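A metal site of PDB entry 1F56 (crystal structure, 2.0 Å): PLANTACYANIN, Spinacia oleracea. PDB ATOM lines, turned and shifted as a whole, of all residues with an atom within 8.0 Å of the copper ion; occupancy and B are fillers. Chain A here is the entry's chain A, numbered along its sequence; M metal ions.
The backbone NH (N) of Phe 76 sits close to the side-chain sulfur (SG) of Cys 74, 3.8 Å away.
The side-chain sulfur (SG) of Cys 74 lies close to the side-chain amide oxygen (OD1) of Asn 35 (3.4 Å).
ND1 of His 79 is bound to the copper ion.
A ring nitrogen (ND1) of His 34 is bound to the copper ion, 2.0 Å away.
SG of Cys 74 is bound to the copper ion.
SD of Met 84 binds the copper ion, at 2.7 Å.
Merely in contact with the copper ion: Gln 33 (3.99 Å).
Five residues have an atom within 4 Å of the copper ion: Gln 33, His 34, Cys 74, His 79 and Met 84.
Along chain A the residues within 4 Å of the copper ion span positions 33 to 84.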
ATOM      1  N   TRP A   7       1.004  22.838  22.412  1.00  0.00           N
ATOM      2  CA  TRP A   7       0.211  21.610  22.284  1.00  0.00           C
ATOM      3  C   TRP A   7       0.170  21.100  20.853  1.00  0.00           C
ATOM      4  O   TRP A   7      -0.628  21.556  20.041  1.00  0.00           O
ATOM      5  CB  TRP A   7      -1.205  21.883  22.807  1.00  0.00           C
ATOM      6  CG  TRP A   7      -2.005  20.654  23.131  1.00  0.00           C
ATOM      7  CD1 TRP A   7      -3.277  20.379  22.705  1.00  0.00           C
ATOM      8  CD2 TRP A   7      -1.617  19.566  23.981  1.00  0.00           C
ATOM      9  NE1 TRP A   7      -3.714  19.206  23.247  1.00  0.00           N
ATOM     10  CE2 TRP A   7      -2.720  18.678  24.037  1.00  0.00           C
ATOM     11  CE3 TRP A   7      -0.457  19.260  24.717  1.00  0.00           C
ATOM     12  CZ2 TRP A   7      -2.703  17.495  24.795  1.00  0.00           C
ATOM     13  CZ3 TRP A   7      -0.438  18.085  25.482  1.00  0.00           C
ATOM     14  CH2 TRP A   7      -1.558  17.209  25.512  1.00  0.00           C
ATOM     15  N   SER A   8       1.039  20.157  20.546  1.00  0.00           N
ATOM     16  CA  SER A   8       1.112  19.583  19.217  1.00  0.00           C
ATOM     17  C   SER A   8       1.600  18.141  19.328  1.00  0.00           C
ATOM     18  O   SER A   8       1.910  17.676  20.418  1.00  0.00           O
ATOM     19  CB  SER A   8       2.072  20.380  18.348  1.00  0.00           C
ATOM     20  OG  SER A   8       2.000  19.928  16.999  1.00  0.00           O
ATOM     21  N   PHE A   9       1.692  17.441  18.199  1.00  0.00           N
ATOM     22  CA  PHE A   9       2.154  16.049  18.232  1.00  0.00           C
ATOM     23  C   PHE A   9       3.497  16.012  18.946  1.00  0.00           C
ATOM     24  O   PHE A   9       3.812  15.064  19.658  1.00  0.00           O
ATOM     25  CB  PHE A   9       2.244  15.506  16.798  1.00  0.00           C
ATOM     26  CG  PHE A   9       0.903  15.326  16.146  1.00  0.00           C
ATOM     27  CD1 PHE A   9       0.156  14.174  16.367  1.00  0.00           C
ATOM     28  CD2 PHE A   9       0.347  16.337  15.356  1.00  0.00           C
ATOM     29  CE1 PHE A   9      -1.115  14.026  15.827  1.00  0.00           C
ATOM     30  CE2 PHE A   9      -0.922  16.206  14.811  1.00  0.00           C
ATOM     31  CZ  PHE A   9      -1.654  15.050  15.047  1.00  0.00           C
ATOM     32  N   TYR A  29      -2.785  26.143  20.769  1.00  0.00           N
ATOM     33  CA  TYR A  29      -2.909  25.416  19.518  1.00  0.00           C
ATOM     34  C   TYR A  29      -4.074  26.024  18.717  1.00  0.00           C
ATOM     35  O   TYR A  29      -4.756  26.943  19.197  1.00  0.00           O
ATOM     36  CB  TYR A  29      -3.183  23.930  19.780  1.00  0.00           C
ATOM     37  CG  TYR A  29      -4.407  23.697  20.654  1.00  0.00           C
ATOM     38  CD1 TYR A  29      -4.326  23.783  22.047  1.00  0.00           C
ATOM     39  CD2 TYR A  29      -5.654  23.442  20.075  1.00  0.00           C
ATOM     40  CE1 TYR A  29      -5.467  23.612  22.841  1.00  0.00           C
ATOM     41  CE2 TYR A  29      -6.807  23.280  20.877  1.00  0.00           C
ATOM     42  CZ  TYR A  29      -6.701  23.364  22.250  1.00  0.00           C
ATOM     43  OH  TYR A  29      -7.827  23.217  23.027  1.00  0.00           O
ATOM     44  N   GLY A  32      -9.956  23.542  17.203  1.00  0.00           N
ATOM     45  CA  GLY A  32     -10.532  22.616  16.250  1.00  0.00           C
ATOM     46  C   GLY A  32      -9.597  21.516  15.793  1.00  0.00           C
ATOM     47  O   GLY A  32     -10.051  20.451  15.365  1.00  0.00           O
ATOM     48  N   GLN A  33      -8.299  21.749  15.889  1.00  0.00           N
ATOM     49  CA  GLN A  33      -7.319  20.757  15.450  1.00  0.00           C
ATOM     50  C   GLN A  33      -6.892  19.779  16.519  1.00  0.00           C
ATOM     51  O   GLN A  33      -6.327  18.716  16.207  1.00  0.00           O
ATOM     52  CB  GLN A  33      -6.087  21.473  14.889  1.00  0.00           C
ATOM     53  CG  GLN A  33      -6.385  22.246  13.598  1.00  0.00           C
ATOM     54  CD  GLN A  33      -5.131  22.642  12.839  1.00  0.00           C
ATOM     55  OE1 GLN A  33      -5.207  23.123  11.709  1.00  0.00           O
ATOM     56  NE2 GLN A  33      -3.972  22.446  13.465  1.00  0.00           N
ATOM     57  N   HIS A  34      -7.133  20.137  17.774  1.00  0.00           N
ATOM     58  CA  HIS A  34      -6.791  19.296  18.928  1.00  0.00           C
ATOM     59  C   HIS A  34      -7.740  19.642  20.080  1.00  0.00           C
ATOM     60  O   HIS A  34      -8.573  20.536  19.984  1.00  0.00           O
ATOM     61  CB  HIS A  34      -5.356  19.585  19.429  1.00  0.00           C
ATOM     62  CG  HIS A  34      -4.281  19.391  18.408  1.00  0.00           C
ATOM     63  ND1 HIS A  34      -3.821  18.149  18.036  1.00  0.00           N
ATOM     64  CD2 HIS A  34      -3.594  20.284  17.649  1.00  0.00           C
ATOM     65  CE1 HIS A  34      -2.908  18.277  17.096  1.00  0.00           C
ATOM     66  NE2 HIS A  34      -2.752  19.567  16.844  1.00  0.00           N
ATOM     67  N   ASN A  35      -7.574  18.904  21.168  1.00  0.00           N
ATOM     68  CA  ASN A  35      -8.301  19.174  22.388  1.00  0.00           C
ATOM     69  C   ASN A  35      -7.369  18.770  23.534  1.00  0.00           C
ATOM     70  O   ASN A  35      -6.302  18.165  23.293  1.00  0.00           O
ATOM     71  CB  ASN A  35      -9.646  18.421  22.438  1.00  0.00           C
ATOM     72  CG  ASN A  35      -9.485  16.929  22.579  1.00  0.00           C
ATOM     73  OD1 ASN A  35      -8.378  16.396  22.646  1.00  0.00           O
ATOM     74  ND2 ASN A  35     -10.615  16.231  22.626  1.00  0.00           N
ATOM     75  N   VAL A  36      -7.742  19.150  24.757  1.00  0.00           N
ATOM     76  CA  VAL A  36      -6.962  18.810  25.936  1.00  0.00           C
ATOM     77  C   VAL A  36      -7.915  18.122  26.910  1.00  0.00           C
ATOM     78  O   VAL A  36      -8.890  18.724  27.344  1.00  0.00           O
ATOM     79  CB  VAL A  36      -6.376  20.047  26.624  1.00  0.00           C
ATOM     80  CG1 VAL A  36      -5.508  19.611  27.811  1.00  0.00           C
ATOM     81  CG2 VAL A  36      -5.583  20.879  25.611  1.00  0.00           C
ATOM     82  N   ILE A  73      -4.099  14.423  27.695  1.00  0.00           N
ATOM     83  CA  ILE A  73      -3.932  13.783  26.382  1.00  0.00           C
ATOM     84  C   ILE A  73      -4.827  14.515  25.391  1.00  0.00           C
ATOM     85  O   ILE A  73      -5.719  15.286  25.793  1.00  0.00           O
ATOM     86  CB  ILE A  73      -4.373  12.262  26.363  1.00  0.00           C
ATOM     87  CG1 ILE A  73      -5.875  12.129  26.615  1.00  0.00           C
ATOM     88  CG2 ILE A  73      -3.593  11.467  27.413  1.00  0.00           C
ATOM     89  CD1 ILE A  73      -6.401  10.694  26.523  1.00  0.00           C
ATOM     90  N   CYS A  74      -4.576  14.321  24.101  1.00  0.00           N
ATOM     91  CA  CYS A  74      -5.451  14.867  23.069  1.00  0.00           C
ATOM     92  C   CYS A  74      -6.198  13.599  22.743  1.00  0.00           C
ATOM     93  O   CYS A  74      -5.579  12.553  22.596  1.00  0.00           O
ATOM     94  CB  CYS A  74      -4.693  15.309  21.816  1.00  0.00           C
ATOM     95  SG  CYS A  74      -5.838  15.810  20.497  1.00  0.00           S
ATOM     96  N   SER A  75      -7.518  13.662  22.626  1.00  0.00           N
ATOM     97  CA  SER A  75      -8.258  12.431  22.362  1.00  0.00           C
ATOM     98  C   SER A  75      -8.628  12.142  20.899  1.00  0.00           C
ATOM     99  O   SER A  75      -9.199  11.094  20.594  1.00  0.00           O
ATOM    100  CB  SER A  75      -9.528  12.423  23.209  1.00  0.00           C
ATOM    101  OG  SER A  75     -10.357  13.489  22.775  1.00  0.00           O
ATOM    102  N   PHE A  76      -8.328  13.052  19.988  1.00  0.00           N
ATOM    103  CA  PHE A  76      -8.678  12.799  18.585  1.00  0.00           C
ATOM    104  C   PHE A  76      -7.915  11.557  18.111  1.00  0.00           C
ATOM    105  O   PHE A  76      -6.813  11.282  18.565  1.00  0.00           O
ATOM    106  CB  PHE A  76      -8.332  14.014  17.714  1.00  0.00           C
ATOM    107  CG  PHE A  76      -9.094  15.276  18.074  1.00  0.00           C
ATOM    108  CD1 PHE A  76     -10.159  15.241  18.968  1.00  0.00           C
ATOM    109  CD2 PHE A  76      -8.778  16.483  17.452  1.00  0.00           C
ATOM    110  CE1 PHE A  76     -10.918  16.412  19.229  1.00  0.00           C
ATOM    111  CE2 PHE A  76      -9.516  17.647  17.716  1.00  0.00           C
ATOM    112  CZ  PHE A  76     -10.597  17.607  18.605  1.00  0.00           C
ATOM    113  N   PRO A  77      -8.525  10.773  17.190  1.00  0.00           N
ATOM    114  CA  PRO A  77      -7.939   9.535  16.639  1.00  0.00           C
ATOM    115  C   PRO A  77      -6.519   9.689  16.153  1.00  0.00           C
ATOM    116  O   PRO A  77      -6.245  10.538  15.319  1.00  0.00           O
ATOM    117  CB  PRO A  77      -8.882   9.194  15.496  1.00  0.00           C
ATOM    118  CG  PRO A  77     -10.179   9.751  15.936  1.00  0.00           C
ATOM    119  CD  PRO A  77      -9.803  11.081  16.534  1.00  0.00           C
ATOM    120  N   GLY A  78      -5.616   8.860  16.680  1.00  0.00           N
ATOM    121  CA  GLY A  78      -4.219   8.897  16.289  1.00  0.00           C
ATOM    122  C   GLY A  78      -3.345   9.935  17.012  1.00  0.00           C
ATOM    123  O   GLY A  78      -2.116   9.838  16.978  1.00  0.00           O
ATOM    124  N   HIS A  79      -3.935  10.905  17.685  1.00  0.00           N
ATOM    125  CA  HIS A  79      -3.102  11.923  18.334  1.00  0.00           C
ATOM    126  C   HIS A  79      -2.378  11.499  19.611  1.00  0.00           C
ATOM    127  O   HIS A  79      -1.193  11.819  19.795  1.00  0.00           O
ATOM    128  CB  HIS A  79      -3.913  13.189  18.596  1.00  0.00           C
ATOM    129  CG  HIS A  79      -4.360  13.880  17.350  1.00  0.00           C
ATOM    130  ND1 HIS A  79      -4.557  15.245  17.286  1.00  0.00           N
ATOM    131  CD2 HIS A  79      -4.706  13.398  16.132  1.00  0.00           C
ATOM    132  CE1 HIS A  79      -5.016  15.568  16.093  1.00  0.00           C
ATOM    133  NE2 HIS A  79      -5.112  14.479  15.371  1.00  0.00           N
ATOM    134  N   CYS A  80      -3.056  10.795  20.507  1.00  0.00           N
ATOM    135  CA  CYS A  80      -2.399  10.353  21.731  1.00  0.00           C
ATOM    136  C   CYS A  80      -1.294   9.344  21.368  1.00  0.00           C
ATOM    137  O   CYS A  80      -0.169   9.409  21.876  1.00  0.00           O
ATOM    138  CB  CYS A  80      -3.427   9.724  22.675  1.00  0.00           C
ATOM    139  SG  CYS A  80      -2.836   9.290  24.342  1.00  0.00           S
ATOM    140  N   MET A  84       0.739  12.892  21.681  1.00  0.00           N
ATOM    141  CA  MET A  84       0.072  13.994  22.350  1.00  0.00           C
ATOM    142  C   MET A  84      -0.444  13.604  23.736  1.00  0.00           C
ATOM    143  O   MET A  84      -1.627  13.359  23.947  1.00  0.00           O
ATOM    144  CB  MET A  84      -1.051  14.552  21.486  1.00  0.00           C
ATOM    145  CG  MET A  84      -0.559  15.389  20.324  1.00  0.00           C
ATOM    146  SD  MET A  84      -1.853  16.410  19.599  1.00  0.00           S
ATOM    147  CE  MET A  84      -1.716  17.956  20.592  1.00  0.00           C
HETATM  148 CU    CU M   1      -4.483  16.436  18.919  1.00  0.00          CU
